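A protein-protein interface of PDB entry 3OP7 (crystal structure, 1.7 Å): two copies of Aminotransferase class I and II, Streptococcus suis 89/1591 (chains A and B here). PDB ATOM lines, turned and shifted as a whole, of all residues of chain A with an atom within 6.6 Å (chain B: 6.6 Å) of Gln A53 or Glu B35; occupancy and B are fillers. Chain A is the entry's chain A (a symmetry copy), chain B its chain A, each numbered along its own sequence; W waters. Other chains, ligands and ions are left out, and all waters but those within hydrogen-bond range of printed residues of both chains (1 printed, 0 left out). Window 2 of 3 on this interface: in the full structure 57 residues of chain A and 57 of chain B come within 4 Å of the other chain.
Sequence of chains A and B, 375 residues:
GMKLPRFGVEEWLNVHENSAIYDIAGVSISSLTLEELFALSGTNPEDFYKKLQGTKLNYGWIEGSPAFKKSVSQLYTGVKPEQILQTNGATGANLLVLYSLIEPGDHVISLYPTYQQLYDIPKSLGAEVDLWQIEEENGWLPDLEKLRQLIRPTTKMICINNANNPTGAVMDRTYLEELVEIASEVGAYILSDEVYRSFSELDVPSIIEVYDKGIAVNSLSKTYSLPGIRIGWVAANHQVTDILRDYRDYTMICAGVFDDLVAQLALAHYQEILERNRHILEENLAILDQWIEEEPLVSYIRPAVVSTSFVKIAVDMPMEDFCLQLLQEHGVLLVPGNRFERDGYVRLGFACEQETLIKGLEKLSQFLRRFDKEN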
ATOM      1  N   PHE A  48     -25.643   3.140  -1.604  1.00  0.00           N
ATOM      2  CA  PHE A  48     -24.461   2.838  -2.381  1.00  0.00           C
ATOM      3  C   PHE A  48     -24.825   2.869  -3.859  1.00  0.00           C
ATOM      4  O   PHE A  48     -24.117   3.471  -4.647  1.00  0.00           O
ATOM      5  CB  PHE A  48     -23.843   1.493  -1.997  1.00  0.00           C
ATOM      6  CG  PHE A  48     -22.635   1.130  -2.795  1.00  0.00           C
ATOM      7  CD1 PHE A  48     -22.763   0.479  -4.019  1.00  0.00           C
ATOM      8  CD2 PHE A  48     -21.363   1.354  -2.300  1.00  0.00           C
ATOM      9  CE1 PHE A  48     -21.646   0.110  -4.749  1.00  0.00           C
ATOM     10  CE2 PHE A  48     -20.249   0.993  -3.015  1.00  0.00           C
ATOM     11  CZ  PHE A  48     -20.387   0.371  -4.265  1.00  0.00           C
ATOM     12  N   TYR A  49     -25.930   2.249  -4.226  1.00  0.00           N
ATOM     13  CA  TYR A  49     -26.328   2.191  -5.638  1.00  0.00           C
ATOM     14  C   TYR A  49     -26.727   3.555  -6.184  1.00  0.00           C
ATOM     15  O   TYR A  49     -26.488   3.839  -7.350  1.00  0.00           O
ATOM     16  CB  TYR A  49     -27.444   1.201  -5.864  1.00  0.00           C
ATOM     17  CG  TYR A  49     -27.014  -0.240  -5.595  1.00  0.00           C
ATOM     18  CD1 TYR A  49     -25.864  -0.759  -6.153  1.00  0.00           C
ATOM     19  CD2 TYR A  49     -27.787  -1.076  -4.789  1.00  0.00           C
ATOM     20  CE1 TYR A  49     -25.452  -2.087  -5.878  1.00  0.00           C
ATOM     21  CE2 TYR A  49     -27.411  -2.369  -4.543  1.00  0.00           C
ATOM     22  CZ  TYR A  49     -26.269  -2.872  -5.060  1.00  0.00           C
ATOM     23  OH  TYR A  49     -25.942  -4.166  -4.797  1.00  0.00           O
ATOM     24  N   LYS A  50     -27.350   4.368  -5.342  1.00  0.00           N
ATOM     25  CA  LYS A  50     -27.717   5.717  -5.740  1.00  0.00           C
ATOM     26  C   LYS A  50     -26.465   6.512  -6.092  1.00  0.00           C
ATOM     27  O   LYS A  50     -26.443   7.186  -7.110  1.00  0.00           O
ATOM     28  CB  LYS A  50     -28.522   6.435  -4.643  1.00  0.00           C
ATOM     29  CG  LYS A  50     -29.179   7.729  -5.141  1.00  0.00           C
ATOM     30  CD  LYS A  50     -30.379   8.150  -4.244  1.00  0.00           C
ATOM     31  CE  LYS A  50     -31.186   9.334  -4.807  1.00  0.00           C
ATOM     32  NZ  LYS A  50     -32.518   9.499  -4.099  1.00  0.00           N
ATOM     33  N   LYS A  51     -25.440   6.434  -5.261  1.00  0.00           N
ATOM     34  CA  LYS A  51     -24.204   7.147  -5.512  1.00  0.00           C
ATOM     35  C   LYS A  51     -23.559   6.605  -6.801  1.00  0.00           C
ATOM     36  O   LYS A  51     -23.210   7.354  -7.702  1.00  0.00           O
ATOM     37  CB  LYS A  51     -23.249   6.991  -4.347  1.00  0.00           C
ATOM     38  CG  LYS A  51     -21.876   7.686  -4.540  1.00  0.00           C
ATOM     39  CD  LYS A  51     -21.231   7.753  -3.190  1.00  0.00           C
ATOM     40  CE  LYS A  51     -19.781   8.159  -3.228  1.00  0.00           C
ATOM     41  NZ  LYS A  51     -19.283   7.964  -1.811  1.00  0.00           N
ATOM     42  N   LEU A  52     -23.451   5.280  -6.884  1.00  0.00           N
ATOM     43  CA  LEU A  52     -22.842   4.638  -8.047  1.00  0.00           C
ATOM     44  C   LEU A  52     -23.538   5.022  -9.336  1.00  0.00           C
ATOM     45  O   LEU A  52     -22.871   5.349 -10.311  1.00  0.00           O
ATOM     46  CB  LEU A  52     -22.880   3.124  -7.898  1.00  0.00           C
ATOM     47  CG  LEU A  52     -22.462   2.347  -9.153  1.00  0.00           C
ATOM     48  CD1 LEU A  52     -20.984   2.579  -9.450  1.00  0.00           C
ATOM     49  CD2 LEU A  52     -22.809   0.823  -8.998  1.00  0.00           C
ATOM     50  N   GLN A  53     -24.856   4.942  -9.336  1.00  0.00           N
ATOM     51  CA  GLN A  53     -25.683   5.034 -10.545  1.00  0.00           C
ATOM     52  C   GLN A  53     -25.544   6.373 -11.276  1.00  0.00           C
ATOM     53  O   GLN A  53     -25.659   6.446 -12.495  1.00  0.00           O
ATOM     54  CB  GLN A  53     -27.141   4.811 -10.156  1.00  0.00           C
ATOM     55  CG  GLN A  53     -28.139   4.886 -11.271  1.00  0.00           C
ATOM     56  CD  GLN A  53     -29.448   4.144 -10.973  1.00  0.00           C
ATOM     57  OE1 GLN A  53     -29.447   3.116 -10.292  1.00  0.00           O
ATOM     58  NE2 GLN A  53     -30.571   4.677 -11.499  1.00  0.00           N
ATOM     59  N   GLY A  54     -25.272   7.410 -10.503  1.00  0.00           N
ATOM     60  CA  GLY A  54     -25.091   8.747 -11.037  1.00  0.00           C
ATOM     61  C   GLY A  54     -23.667   9.201 -11.236  1.00  0.00           C
ATOM     62  O   GLY A  54     -23.451  10.368 -11.640  1.00  0.00           O
ATOM     63  N   THR A  55     -22.706   8.308 -10.994  1.00  0.00           N
ATOM     64  CA  THR A  55     -21.286   8.617 -11.155  1.00  0.00           C
ATOM     65  C   THR A  55     -20.890   8.395 -12.615  1.00  0.00           C
ATOM     66  O   THR A  55     -21.066   7.320 -13.152  1.00  0.00           O
ATOM     67  CB  THR A  55     -20.417   7.819 -10.183  1.00  0.00           C
ATOM     68  OG1 THR A  55     -20.811   8.130  -8.848  1.00  0.00           O
ATOM     69  CG2 THR A  55     -18.926   8.118 -10.350  1.00  0.00           C
ATOM     70  N   LYS A  56     -20.316   9.406 -13.245  1.00  0.00           N
ATOM     71  CA  LYS A  56     -19.803   9.233 -14.613  1.00  0.00           C
ATOM     72  C   LYS A  56     -18.724   8.143 -14.621  1.00  0.00           C
ATOM     73  O   LYS A  56     -17.803   8.139 -13.789  1.00  0.00           O
ATOM     74  CB  LYS A  56     -19.202  10.534 -15.111  1.00  0.00           C
ATOM     75  CG  LYS A  56     -20.237  11.563 -15.456  1.00  0.00           C
ATOM     76  CD  LYS A  56     -19.576  12.833 -15.945  1.00  0.00           C
ATOM     77  CE  LYS A  56     -20.525  14.028 -15.938  1.00  0.00           C
ATOM     78  NZ  LYS A  56     -21.765  13.801 -16.739  1.00  0.00           N
ATOM     79  N   LEU B  32     -20.620   7.871 -20.063  1.00  0.00           N
ATOM     80  CA  LEU B  32     -21.928   7.425 -19.578  1.00  0.00           C
ATOM     81  C   LEU B  32     -21.905   7.253 -18.089  1.00  0.00           C
ATOM     82  O   LEU B  32     -20.884   6.832 -17.509  1.00  0.00           O
ATOM     83  CB  LEU B  32     -22.284   6.085 -20.236  1.00  0.00           C
ATOM     84  CG  LEU B  32     -22.761   6.162 -21.704  1.00  0.00           C
ATOM     85  CD1 LEU B  32     -22.673   4.725 -22.353  1.00  0.00           C
ATOM     86  CD2 LEU B  32     -24.143   6.728 -21.751  1.00  0.00           C
ATOM     87  N   THR B  33     -23.039   7.508 -17.470  1.00  0.00           N
ATOM     88  CA  THR B  33     -23.307   6.960 -16.141  1.00  0.00           C
ATOM     89  C   THR B  33     -24.054   5.620 -16.275  1.00  0.00           C
ATOM     90  O   THR B  33     -24.640   5.322 -17.310  1.00  0.00           O
ATOM     91  CB  THR B  33     -24.178   7.864 -15.307  1.00  0.00           C
ATOM     92  OG1 THR B  33     -25.474   7.980 -15.948  1.00  0.00           O
ATOM     93  CG2 THR B  33     -23.542   9.280 -15.104  1.00  0.00           C
ATOM     94  N   LEU B  34     -24.071   4.824 -15.211  1.00  0.00           N
ATOM     95  CA  LEU B  34     -24.843   3.584 -15.218  1.00  0.00           C
ATOM     96  C   LEU B  34     -26.309   3.893 -15.489  1.00  0.00           C
ATOM     97  O   LEU B  34     -26.953   3.214 -16.274  1.00  0.00           O
ATOM     98  CB  LEU B  34     -24.651   2.843 -13.874  1.00  0.00           C
ATOM     99  CG  LEU B  34     -24.767   1.335 -13.903  1.00  0.00           C
ATOM    100  CD1 LEU B  34     -23.948   0.734 -15.052  1.00  0.00           C
ATOM    101  CD2 LEU B  34     -24.353   0.787 -12.516  1.00  0.00           C
ATOM    102  N   GLU B  35     -26.823   4.943 -14.854  1.00  0.00           N
ATOM    103  CA  GLU B  35     -28.201   5.401 -15.070  1.00  0.00           C
ATOM    104  C   GLU B  35     -28.506   5.600 -16.560  1.00  0.00           C
ATOM    105  O   GLU B  35     -29.517   5.125 -17.052  1.00  0.00           O
ATOM    106  CB  GLU B  35     -28.420   6.737 -14.346  1.00  0.00           C
ATOM    107  CG  GLU B  35     -29.708   7.489 -14.713  1.00  0.00           C
ATOM    108  CD  GLU B  35     -30.790   7.396 -13.679  1.00  0.00           C
ATOM    109  OE1 GLU B  35     -30.478   7.294 -12.463  1.00  0.00           O
ATOM    110  OE2 GLU B  35     -31.973   7.466 -14.102  1.00  0.00           O
ATOM    111  N   GLU B  36     -27.632   6.317 -17.252  1.00  0.00           N
ATOM    112  CA  GLU B  36     -27.808   6.570 -18.679  1.00  0.00           C
ATOM    113  C   GLU B  36     -27.683   5.275 -19.479  1.00  0.00           C
ATOM    114  O   GLU B  36     -28.408   5.071 -20.457  1.00  0.00           O
ATOM    115  CB  GLU B  36     -26.826   7.643 -19.220  1.00  0.00           C
ATOM    116  CG  GLU B  36     -27.261   8.207 -20.589  1.00  0.00           C
ATOM    117  CD  GLU B  36     -26.331   9.219 -21.259  1.00  0.00           C
ATOM    118  OE1 GLU B  36     -25.353   9.697 -20.639  1.00  0.00           O
ATOM    119  OE2 GLU B  36     -26.608   9.533 -22.447  1.00  0.00           O
ATOM    120  N   LEU B  37     -26.749   4.402 -19.091  1.00  0.00           N
ATOM    121  CA  LEU B  37     -26.633   3.112 -19.775  1.00  0.00           C
ATOM    122  C   LEU B  37     -27.877   2.238 -19.600  1.00  0.00           C
ATOM    123  O   LEU B  37     -28.354   1.636 -20.575  1.00  0.00           O
ATOM    124  CB  LEU B  37     -25.419   2.330 -19.312  1.00  0.00           C
ATOM    125  CG  LEU B  37     -25.157   0.973 -19.962  1.00  0.00           C
ATOM    126  CD1 LEU B  37     -25.013   1.064 -21.511  1.00  0.00           C
ATOM    127  CD2 LEU B  37     -23.920   0.272 -19.299  1.00  0.00           C
ATOM    128  N   PHE B  38     -28.449   2.220 -18.400  1.00  0.00           N
ATOM    129  CA  PHE B  38     -29.690   1.493 -18.195  1.00  0.00           C
ATOM    130  C   PHE B  38     -30.788   2.064 -19.087  1.00  0.00           C
ATOM    131  O   PHE B  38     -31.548   1.316 -19.704  1.00  0.00           O
ATOM    132  CB  PHE B  38     -30.134   1.576 -16.740  1.00  0.00           C
ATOM    133  CG  PHE B  38     -29.257   0.812 -15.760  1.00  0.00           C
ATOM    134  CD1 PHE B  38     -28.674  -0.386 -16.105  1.00  0.00           C
ATOM    135  CD2 PHE B  38     -29.111   1.266 -14.461  1.00  0.00           C
ATOM    136  CE1 PHE B  38     -27.930  -1.093 -15.182  1.00  0.00           C
ATOM    137  CE2 PHE B  38     -28.360   0.559 -13.539  1.00  0.00           C
ATOM    138  CZ  PHE B  38     -27.776  -0.624 -13.899  1.00  0.00           C
ATOM    139  N   ALA B  39     -30.866   3.394 -19.153  1.00  0.00           N
ATOM    140  CA  ALA B  39     -31.910   4.058 -19.932  1.00  0.00           C
ATOM    141  C   ALA B  39     -31.809   3.759 -21.422  1.00  0.00           C
ATOM    142  O   ALA B  39     -32.803   3.415 -22.055  1.00  0.00           O
ATOM    143  CB  ALA B  39     -31.912   5.589 -19.688  1.00  0.00           C
ATOM    144  N   LEU B  40     -30.620   3.886 -22.000  1.00  0.00           N
ATOM    145  CA  LEU B  40     -30.504   3.656 -23.428  1.00  0.00           C
ATOM    146  C   LEU B  40     -30.641   2.158 -23.785  1.00  0.00           C
ATOM    147  O   LEU B  40     -31.049   1.815 -24.897  1.00  0.00           O
ATOM    148  CB  LEU B  40     -29.247   4.322 -24.007  1.00  0.00           C
ATOM    149  CG  LEU B  40     -27.902   3.809 -23.578  1.00  0.00           C
ATOM    150  CD1 LEU B  40     -27.669   2.483 -24.313  1.00  0.00           C
ATOM    151  CD2 LEU B  40     -26.761   4.829 -23.876  1.00  0.00           C
ATOM    152  N   PRO B  45     -32.854  -1.361 -13.575  1.00  0.00           N
ATOM    153  CA  PRO B  45     -31.701  -1.253 -12.706  1.00  0.00           C
ATOM    154  C   PRO B  45     -31.721  -2.297 -11.579  1.00  0.00           C
ATOM    155  O   PRO B  45     -30.679  -2.868 -11.259  1.00  0.00           O
ATOM    156  CB  PRO B  45     -31.821   0.175 -12.149  1.00  0.00           C
ATOM    157  CG  PRO B  45     -32.510   0.917 -13.194  1.00  0.00           C
ATOM    158  CD  PRO B  45     -33.524  -0.047 -13.739  1.00  0.00           C
ATOM    159  N   TYR B  49     -28.812  -4.911 -10.359  1.00  0.00           N
ATOM    160  CA  TYR B  49     -28.219  -4.873  -9.016  1.00  0.00           C
ATOM    161  C   TYR B  49     -28.415  -6.178  -8.258  1.00  0.00           C
ATOM    162  O   TYR B  49     -27.551  -6.570  -7.485  1.00  0.00           O
ATOM    163  CB  TYR B  49     -28.756  -3.721  -8.203  1.00  0.00           C
ATOM    164  CG  TYR B  49     -28.350  -2.361  -8.769  1.00  0.00           C
ATOM    165  CD1 TYR B  49     -27.037  -2.083  -9.087  1.00  0.00           C
ATOM    166  CD2 TYR B  49     -29.299  -1.357  -8.961  1.00  0.00           C
ATOM    167  CE1 TYR B  49     -26.668  -0.831  -9.640  1.00  0.00           C
ATOM    168  CE2 TYR B  49     -28.946  -0.136  -9.467  1.00  0.00           C
ATOM    169  CZ  TYR B  49     -27.667   0.131  -9.812  1.00  0.00           C
ATOM    170  OH  TYR B  49     -27.361   1.363 -10.300  1.00  0.00           O
HETATM  171  O   HOH W   1     -22.210   4.987 -13.013  1.00  0.00           O
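Among the printed residues, pairs that only touch across the chains: Tyr A49 with Tyr B49 (3.4 Å), Gln A53 with Thr B33 (3.5 Å), Gln A53 with Leu B34 (3.5 Å), Gly A54 with Thr B33 (3.6 Å), Thr A55 with Thr B33 (3.7 Å), Lys A56 with Thr B33 (3.7 Å), Lys A56 with Leu B32 (3.8 Å) and Leu A52 with Leu B34 (3.8 Å).
Tyr A49 touches its own counterpart, Tyr B49. Position printed for both chains: 49. Of the 10 pairs that touch across the chains among the printed residues, 1 has its exchanged pair printed and touching as well.
Printed residues of chain B that touch a printed residue of chain A: Leu B32, Thr B33, Leu B34, Glu B35 and Tyr B49. Hydrophobic or aromatic side chains of chain B within 4 Å of the printed part of chain A: Leu B34 and Tyr B49. Along chain B the printed residues that touch a printed residue of chain A span positions 32 to 49. Printed residues of chain A that touch a printed residue of chain B: Tyr A49, Leu A52, Gln A53, Gly A54, Thr A55 and Lys A56. Among the printed residues, 10 pairs touch across the chains. Among the printed residues, no Asp or Glu carboxylate lies within 4 Å of a Lys or Arg side-chain nitrogen of the other chain.
Of the printed residues of chain B, Tyr A49 touches Tyr B49. Lys A50 touches none of the printed residues of chain B. Of the printed residues of chain B, Thr A55 touches Thr B33. Of the printed residues of chain A, Thr B33 touches Gln A53, Gly A54, Thr A55 and Lys A56. Leu B40 touches none of the printed residues of chain A. The nearest residue of chain B that does not touch Gln A53 is Pro B45 (4.2 Å). The nearest residue of chain A that does not touch Glu B35 is Gly A54 (5.0 Å).
Water W1 lies within hydrogen-bond range of the backbone carbonyl oxygen of Thr A55 (2.6 Å), the backbone carbonyl oxygen of Leu A52 (2.8 Å) and the backbone NH of Leu B34 (2.9 Å).
The side-chain hydroxyl of Thr B33 sits close to the backbone NH of Glu B35, at 3.5 Å. The side-chain hydroxyl of Thr A55 lies within hydrogen-bond range of the backbone carbonyl oxygen of Lys A51, at 2.8 Å. The side-chain hydroxyl (OG1) of Thr B33 sits at hydrogen-bond distance from the backbone NH (N) of Glu B36, 3.0 Å away.
OH of Tyr B49 is in hydrogen-bond range of OE1 of Gln A53. OE1 of Glu B35 sits at hydrogen-bond distance from NE2 of Gln A53 (2.8 Å).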
